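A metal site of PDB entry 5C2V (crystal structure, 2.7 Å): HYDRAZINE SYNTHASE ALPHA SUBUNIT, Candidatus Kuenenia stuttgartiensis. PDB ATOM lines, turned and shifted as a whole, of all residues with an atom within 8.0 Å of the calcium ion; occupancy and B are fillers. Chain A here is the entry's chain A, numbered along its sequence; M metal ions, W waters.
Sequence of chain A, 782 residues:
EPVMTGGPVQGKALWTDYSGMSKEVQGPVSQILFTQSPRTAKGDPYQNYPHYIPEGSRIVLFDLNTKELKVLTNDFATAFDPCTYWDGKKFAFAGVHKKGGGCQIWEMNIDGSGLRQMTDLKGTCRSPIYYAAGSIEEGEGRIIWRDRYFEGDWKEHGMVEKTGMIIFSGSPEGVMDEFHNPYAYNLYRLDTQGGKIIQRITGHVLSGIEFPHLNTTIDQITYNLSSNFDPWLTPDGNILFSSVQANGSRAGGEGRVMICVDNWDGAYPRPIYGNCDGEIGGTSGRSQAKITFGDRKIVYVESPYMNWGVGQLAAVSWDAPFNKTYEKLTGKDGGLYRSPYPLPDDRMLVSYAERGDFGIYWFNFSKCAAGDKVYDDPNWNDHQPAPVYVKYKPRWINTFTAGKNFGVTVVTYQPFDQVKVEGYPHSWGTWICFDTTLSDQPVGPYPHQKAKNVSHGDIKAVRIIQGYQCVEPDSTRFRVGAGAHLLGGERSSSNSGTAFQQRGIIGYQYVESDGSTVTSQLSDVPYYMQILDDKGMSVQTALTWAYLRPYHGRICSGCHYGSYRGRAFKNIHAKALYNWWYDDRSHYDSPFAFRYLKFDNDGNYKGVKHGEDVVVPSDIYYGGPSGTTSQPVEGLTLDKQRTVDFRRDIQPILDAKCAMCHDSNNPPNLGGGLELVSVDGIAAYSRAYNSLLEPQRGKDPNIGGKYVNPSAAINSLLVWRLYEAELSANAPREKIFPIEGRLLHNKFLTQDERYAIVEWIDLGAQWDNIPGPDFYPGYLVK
The backbone carbonyl oxygen (O) of Ile 770 lies close to the side-chain amide nitrogen (NE2) of Gln 502. The side-chain carboxylate (OD1) of Asp 774 lies within salt-bridge range of the guanidinium group (NH1) of Arg 647 (3.4 Å). NH1 of Arg 477 is in hydrogen-bond range of O of Asp 774. The side-chain carboxylate of Asp 774 sits at hydrogen-bond distance from the backbone NH of Tyr 776, at 3.1 Å. The side-chain amide nitrogen (NE2) of Gln 502 is in hydrogen-bond range of the backbone carbonyl oxygen (O) of Asp 768 (2.9 Å). N of Asp 768 lies within hydrogen-bond range of O of Asn 495 (2.7 Å). NH1 of Arg 647 lies close to OD2 of Asp 768 (2.8 Å). The backbone NH of Gly 772 lies within hydrogen-bond range of the side-chain carboxylate of Glu 472 (3.4 Å).
The nearest printed residue that does not touch the calcium ion is Gln 502 (4.1 Å).
The calcium ion is bound by O of Ile 770 (2.2 Å), OD2 of Asp 774 (2.3 Å), OD2 of Asp 768 (2.4 Å), O of Gly 772 (2.4 Å), water W1 (2.4 Å), water W2 (2.4 Å) and OD1 of Asp 768 (2.5 Å). The calcium ion has seven donor atoms within binding distance.
Water W2 lies within hydrogen-bond range of the side-chain amide oxygen (OD1) of Asn 495 (2.6 Å), the side-chain carboxylate (OE2) of Glu 472 (2.6 Å), the side-chain amide nitrogen (NE2) of Gln 502 (3.1 Å) and the backbone NH (N) of Gly 772 (3.5 Å).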
ATOM      1  N   VAL A 471      -8.758 -22.044 -10.762  1.00  0.00           N
ATOM      2  CA  VAL A 471      -7.787 -22.498 -11.748  1.00  0.00           C
ATOM      3  C   VAL A 471      -6.377 -22.446 -11.147  1.00  0.00           C
ATOM      4  O   VAL A 471      -5.879 -21.386 -10.759  1.00  0.00           O
ATOM      5  CB  VAL A 471      -7.865 -21.673 -13.058  1.00  0.00           C
ATOM      6  CG1 VAL A 471      -9.219 -21.880 -13.725  1.00  0.00           C
ATOM      7  CG2 VAL A 471      -7.650 -20.189 -12.806  1.00  0.00           C
ATOM      8  N   GLU A 472      -5.761 -23.612 -11.044  1.00  0.00           N
ATOM      9  CA  GLU A 472      -4.458 -23.718 -10.403  1.00  0.00           C
ATOM     10  C   GLU A 472      -3.510 -24.573 -11.223  1.00  0.00           C
ATOM     11  O   GLU A 472      -3.395 -25.776 -11.000  1.00  0.00           O
ATOM     12  CB  GLU A 472      -4.602 -24.296  -8.991  1.00  0.00           C
ATOM     13  CG  GLU A 472      -5.407 -23.413  -8.026  1.00  0.00           C
ATOM     14  CD  GLU A 472      -4.695 -22.125  -7.686  1.00  0.00           C
ATOM     15  OE1 GLU A 472      -3.465 -22.041  -7.871  1.00  0.00           O
ATOM     16  OE2 GLU A 472      -5.370 -21.175  -7.224  1.00  0.00           O
ATOM     17  N   ARG A 477       1.785 -25.137  -5.645  1.00  0.00           N
ATOM     18  CA  ARG A 477       1.307 -23.978  -4.888  1.00  0.00           C
ATOM     19  C   ARG A 477      -0.151 -24.073  -4.427  1.00  0.00           C
ATOM     20  O   ARG A 477      -0.676 -23.128  -3.836  1.00  0.00           O
ATOM     21  CB  ARG A 477       1.509 -22.700  -5.709  1.00  0.00           C
ATOM     22  CG  ARG A 477       2.977 -22.333  -5.905  1.00  0.00           C
ATOM     23  CD  ARG A 477       3.159 -20.838  -6.071  1.00  0.00           C
ATOM     24  NE  ARG A 477       2.581 -20.094  -4.968  1.00  0.00           N
ATOM     25  CZ  ARG A 477       2.600 -18.763  -4.867  1.00  0.00           C
ATOM     26  NH1 ARG A 477       3.178 -18.040  -5.806  1.00  0.00           N
ATOM     27  NH2 ARG A 477       2.040 -18.163  -3.821  1.00  0.00           N
ATOM     28  N   PHE A 478      -0.810 -25.194  -4.710  1.00  0.00           N
ATOM     29  CA  PHE A 478      -2.208 -25.364  -4.309  1.00  0.00           C
ATOM     30  C   PHE A 478      -2.451 -26.716  -3.636  1.00  0.00           C
ATOM     31  O   PHE A 478      -1.999 -27.748  -4.125  1.00  0.00           O
ATOM     32  CB  PHE A 478      -3.139 -25.197  -5.514  1.00  0.00           C
ATOM     33  CG  PHE A 478      -4.596 -25.287  -5.169  1.00  0.00           C
ATOM     34  CD1 PHE A 478      -5.237 -24.243  -4.514  1.00  0.00           C
ATOM     35  CD2 PHE A 478      -5.339 -26.415  -5.493  1.00  0.00           C
ATOM     36  CE1 PHE A 478      -6.578 -24.319  -4.199  1.00  0.00           C
ATOM     37  CE2 PHE A 478      -6.680 -26.492  -5.177  1.00  0.00           C
ATOM     38  CZ  PHE A 478      -7.302 -25.447  -4.534  1.00  0.00           C
ATOM     39  N   SER A 494      -6.097 -24.240   0.044  1.00  0.00           N
ATOM     40  CA  SER A 494      -5.025 -23.264   0.278  1.00  0.00           C
ATOM     41  C   SER A 494      -5.549 -21.842   0.115  1.00  0.00           C
ATOM     42  O   SER A 494      -5.019 -20.907   0.715  1.00  0.00           O
ATOM     43  CB  SER A 494      -3.858 -23.523  -0.679  1.00  0.00           C
ATOM     44  OG  SER A 494      -2.909 -22.471  -0.603  1.00  0.00           O
ATOM     45  N   ASN A 495      -6.582 -21.686  -0.710  1.00  0.00           N
ATOM     46  CA  ASN A 495      -7.180 -20.376  -0.964  1.00  0.00           C
ATOM     47  C   ASN A 495      -8.139 -19.916   0.135  1.00  0.00           C
ATOM     48  O   ASN A 495      -8.264 -18.722   0.382  1.00  0.00           O
ATOM     49  CB  ASN A 495      -7.902 -20.380  -2.300  1.00  0.00           C
ATOM     50  CG  ASN A 495      -6.960 -20.508  -3.484  1.00  0.00           C
ATOM     51  OD1 ASN A 495      -5.805 -20.075  -3.411  1.00  0.00           O
ATOM     52  ND2 ASN A 495      -7.438 -21.099  -4.565  1.00  0.00           N
ATOM     53  N   GLN A 502     -12.962 -18.568  -4.381  1.00  0.00           N
ATOM     54  CA  GLN A 502     -12.535 -17.198  -4.621  1.00  0.00           C
ATOM     55  C   GLN A 502     -13.628 -16.334  -5.272  1.00  0.00           C
ATOM     56  O   GLN A 502     -14.288 -16.769  -6.220  1.00  0.00           O
ATOM     57  CB  GLN A 502     -11.278 -17.195  -5.488  1.00  0.00           C
ATOM     58  CG  GLN A 502     -10.148 -18.015  -4.888  1.00  0.00           C
ATOM     59  CD  GLN A 502      -8.944 -18.118  -5.799  1.00  0.00           C
ATOM     60  OE1 GLN A 502      -8.959 -18.850  -6.787  1.00  0.00           O
ATOM     61  NE2 GLN A 502      -7.880 -17.398  -5.456  1.00  0.00           N
ATOM     62  N   ASP A 645      -8.630  -9.300  -0.278  1.00  0.00           N
ATOM     63  CA  ASP A 645      -7.687 -10.362   0.025  1.00  0.00           C
ATOM     64  C   ASP A 645      -7.177 -10.211   1.456  1.00  0.00           C
ATOM     65  O   ASP A 645      -6.839  -9.107   1.882  1.00  0.00           O
ATOM     66  CB  ASP A 645      -6.513 -10.345  -0.970  1.00  0.00           C
ATOM     67  CG  ASP A 645      -5.677 -11.602  -0.900  1.00  0.00           C
ATOM     68  OD1 ASP A 645      -4.748 -11.659  -0.065  1.00  0.00           O
ATOM     69  OD2 ASP A 645      -5.943 -12.531  -1.697  1.00  0.00           O
ATOM     70  N   ARG A 647      -4.427 -11.262   2.897  1.00  0.00           N
ATOM     71  CA  ARG A 647      -2.998 -10.955   2.991  1.00  0.00           C
ATOM     72  C   ARG A 647      -2.695  -9.516   2.601  1.00  0.00           C
ATOM     73  O   ARG A 647      -1.905  -8.833   3.258  1.00  0.00           O
ATOM     74  CB  ARG A 647      -2.214 -11.915   2.105  1.00  0.00           C
ATOM     75  CG  ARG A 647      -2.591 -13.377   2.309  1.00  0.00           C
ATOM     76  CD  ARG A 647      -2.260 -14.219   1.082  1.00  0.00           C
ATOM     77  NE  ARG A 647      -2.988 -13.764  -0.105  1.00  0.00           N
ATOM     78  CZ  ARG A 647      -2.938 -14.377  -1.289  1.00  0.00           C
ATOM     79  NH1 ARG A 647      -2.206 -15.465  -1.441  1.00  0.00           N
ATOM     80  NH2 ARG A 647      -3.635 -13.894  -2.303  1.00  0.00           N
ATOM     81  N   TRP A 767      -8.820 -16.549   2.059  1.00  0.00           N
ATOM     82  CA  TRP A 767      -7.416 -16.244   2.309  1.00  0.00           C
ATOM     83  C   TRP A 767      -6.803 -15.709   1.023  1.00  0.00           C
ATOM     84  O   TRP A 767      -6.330 -14.574   0.981  1.00  0.00           O
ATOM     85  CB  TRP A 767      -6.689 -17.499   2.811  1.00  0.00           C
ATOM     86  CG  TRP A 767      -5.185 -17.457   2.681  1.00  0.00           C
ATOM     87  CD1 TRP A 767      -4.431 -18.022   1.696  1.00  0.00           C
ATOM     88  CD2 TRP A 767      -4.261 -16.832   3.579  1.00  0.00           C
ATOM     89  NE1 TRP A 767      -3.098 -17.787   1.919  1.00  0.00           N
ATOM     90  CE2 TRP A 767      -2.968 -17.055   3.065  1.00  0.00           C
ATOM     91  CE3 TRP A 767      -4.398 -16.089   4.763  1.00  0.00           C
ATOM     92  CZ2 TRP A 767      -1.819 -16.573   3.700  1.00  0.00           C
ATOM     93  CZ3 TRP A 767      -3.256 -15.621   5.385  1.00  0.00           C
ATOM     94  CH2 TRP A 767      -1.991 -15.858   4.855  1.00  0.00           C
ATOM     95  N   ASP A 768      -6.807 -16.538  -0.023  1.00  0.00           N
ATOM     96  CA  ASP A 768      -6.344 -16.123  -1.335  1.00  0.00           C
ATOM     97  C   ASP A 768      -7.550 -15.831  -2.230  1.00  0.00           C
ATOM     98  O   ASP A 768      -8.236 -16.743  -2.678  1.00  0.00           O
ATOM     99  CB  ASP A 768      -5.467 -17.214  -1.955  1.00  0.00           C
ATOM    100  CG  ASP A 768      -4.633 -16.722  -3.126  1.00  0.00           C
ATOM    101  OD1 ASP A 768      -5.121 -15.884  -3.916  1.00  0.00           O
ATOM    102  OD2 ASP A 768      -3.482 -17.181  -3.261  1.00  0.00           O
ATOM    103  N   ASN A 769      -7.808 -14.551  -2.493  1.00  0.00           N
ATOM    104  CA  ASN A 769      -8.882 -14.151  -3.387  1.00  0.00           C
ATOM    105  C   ASN A 769      -8.390 -13.819  -4.797  1.00  0.00           C
ATOM    106  O   ASN A 769      -9.182 -13.451  -5.667  1.00  0.00           O
ATOM    107  CB  ASN A 769      -9.663 -12.960  -2.817  1.00  0.00           C
ATOM    108  CG  ASN A 769     -10.951 -13.384  -2.136  1.00  0.00           C
ATOM    109  OD1 ASN A 769     -11.478 -14.470  -2.402  1.00  0.00           O
ATOM    110  ND2 ASN A 769     -11.463 -12.532  -1.264  1.00  0.00           N
ATOM    111  N   ILE A 770      -7.094 -13.943  -5.012  1.00  0.00           N
ATOM    112  CA  ILE A 770      -6.510 -13.750  -6.320  1.00  0.00           C
ATOM    113  C   ILE A 770      -6.271 -15.110  -6.982  1.00  0.00           C
ATOM    114  O   ILE A 770      -5.403 -15.857  -6.542  1.00  0.00           O
ATOM    115  CB  ILE A 770      -5.191 -12.968  -6.259  1.00  0.00           C
ATOM    116  CG1 ILE A 770      -5.419 -11.591  -5.622  1.00  0.00           C
ATOM    117  CG2 ILE A 770      -4.582 -12.818  -7.644  1.00  0.00           C
ATOM    118  CD1 ILE A 770      -4.161 -10.750  -5.529  1.00  0.00           C
ATOM    119  N   PRO A 771      -7.059 -15.432  -8.016  1.00  0.00           N
ATOM    120  CA  PRO A 771      -7.017 -16.727  -8.706  1.00  0.00           C
ATOM    121  C   PRO A 771      -5.637 -17.054  -9.263  1.00  0.00           C
ATOM    122  O   PRO A 771      -4.954 -16.173  -9.801  1.00  0.00           O
ATOM    123  CB  PRO A 771      -8.029 -16.552  -9.845  1.00  0.00           C
ATOM    124  CG  PRO A 771      -8.965 -15.505  -9.349  1.00  0.00           C
ATOM    125  CD  PRO A 771      -8.117 -14.555  -8.558  1.00  0.00           C
ATOM    126  N   GLY A 772      -5.231 -18.317  -9.146  1.00  0.00           N
ATOM    127  CA  GLY A 772      -3.934 -18.753  -9.620  1.00  0.00           C
ATOM    128  C   GLY A 772      -2.811 -18.363  -8.682  1.00  0.00           C
ATOM    129  O   GLY A 772      -3.015 -17.571  -7.768  1.00  0.00           O
ATOM    130  N   PRO A 773      -1.618 -18.932  -8.909  1.00  0.00           N
ATOM    131  CA  PRO A 773      -0.440 -18.599  -8.096  1.00  0.00           C
ATOM    132  C   PRO A 773      -0.056 -17.132  -8.215  1.00  0.00           C
ATOM    133  O   PRO A 773       0.052 -16.606  -9.330  1.00  0.00           O
ATOM    134  CB  PRO A 773       0.655 -19.495  -8.685  1.00  0.00           C
ATOM    135  CG  PRO A 773      -0.073 -20.592  -9.379  1.00  0.00           C
ATOM    136  CD  PRO A 773      -1.326 -19.972  -9.899  1.00  0.00           C
ATOM    137  N   ASP A 774       0.156 -16.470  -7.083  1.00  0.00           N
ATOM    138  CA  ASP A 774       0.566 -15.066  -7.069  1.00  0.00           C
ATOM    139  C   ASP A 774       1.766 -14.857  -6.149  1.00  0.00           C
ATOM    140  O   ASP A 774       2.312 -15.808  -5.598  1.00  0.00           O
ATOM    141  CB  ASP A 774      -0.603 -14.170  -6.646  1.00  0.00           C
ATOM    142  CG  ASP A 774      -1.275 -14.650  -5.371  1.00  0.00           C
ATOM    143  OD1 ASP A 774      -0.706 -14.449  -4.276  1.00  0.00           O
ATOM    144  OD2 ASP A 774      -2.394 -15.216  -5.476  1.00  0.00           O
ATOM    145  N   PHE A 775       2.165 -13.602  -5.999  1.00  0.00           N
ATOM    146  CA  PHE A 775       3.367 -13.265  -5.234  1.00  0.00           C
ATOM    147  C   PHE A 775       3.128 -13.265  -3.724  1.00  0.00           C
ATOM    148  O   PHE A 775       4.083 -13.372  -2.942  1.00  0.00           O
ATOM    149  CB  PHE A 775       3.911 -11.904  -5.684  1.00  0.00           C
ATOM    150  CG  PHE A 775       4.432 -11.885  -7.084  1.00  0.00           C
ATOM    151  CD1 PHE A 775       5.022 -13.023  -7.625  1.00  0.00           C
ATOM    152  CD2 PHE A 775       4.338 -10.758  -7.865  1.00  0.00           C
ATOM    153  CE1 PHE A 775       5.517 -13.016  -8.919  1.00  0.00           C
ATOM    154  CE2 PHE A 775       4.824 -10.742  -9.164  1.00  0.00           C
ATOM    155  CZ  PHE A 775       5.410 -11.869  -9.684  1.00  0.00           C
ATOM    156  N   TYR A 776       1.880 -13.133  -3.324  1.00  0.00           N
ATOM    157  CA  TYR A 776       1.533 -13.085  -1.902  1.00  0.00           C
ATOM    158  C   TYR A 776       1.711 -14.447  -1.240  1.00  0.00           C
ATOM    159  O   TYR A 776       1.557 -15.479  -1.890  1.00  0.00           O
ATOM    160  CB  TYR A 776       0.096 -12.579  -1.726  1.00  0.00           C
ATOM    161  CG  TYR A 776      -0.079 -11.128  -2.125  1.00  0.00           C
ATOM    162  CD1 TYR A 776      -0.375 -10.779  -3.445  1.00  0.00           C
ATOM    163  CD2 TYR A 776       0.049 -10.110  -1.195  1.00  0.00           C
ATOM    164  CE1 TYR A 776      -0.531  -9.457  -3.807  1.00  0.00           C
ATOM    165  CE2 TYR A 776      -0.104  -8.781  -1.551  1.00  0.00           C
ATOM    166  CZ  TYR A 776      -0.399  -8.468  -2.863  1.00  0.00           C
ATOM    167  OH  TYR A 776      -0.555  -7.146  -3.226  1.00  0.00           O
ATOM    168  N   PRO A 777       2.063 -14.451   0.068  1.00  0.00           N
ATOM    169  CA  PRO A 777       2.348 -15.675   0.835  1.00  0.00           C
ATOM    170  C   PRO A 777       1.269 -16.742   0.720  1.00  0.00           C
ATOM    171  O   PRO A 777       0.078 -16.422   0.650  1.00  0.00           O
ATOM    172  CB  PRO A 777       2.450 -15.162   2.266  1.00  0.00           C
ATOM    173  CG  PRO A 777       2.936 -13.765   2.122  1.00  0.00           C
ATOM    174  CD  PRO A 777       2.272 -13.238   0.869  1.00  0.00           C
ATOM    175  N   GLY A 778       1.682 -18.011   0.714  1.00  0.00           N
ATOM    176  CA  GLY A 778       0.753 -19.116   0.607  1.00  0.00           C
ATOM    177  C   GLY A 778       1.424 -20.472   0.588  1.00  0.00           C
ATOM    178  O   GLY A 778       2.640 -20.582   0.778  1.00  0.00           O
HETATM  179 CA    CA M   1      -3.796 -17.090  -5.594  1.00  0.00          CA
HETATM  180  O   HOH W   1      -2.053 -18.424  -4.656  1.00  0.00           O
HETATM  181  O   HOH W   2      -5.214 -19.011  -5.715  1.00  0.00           O
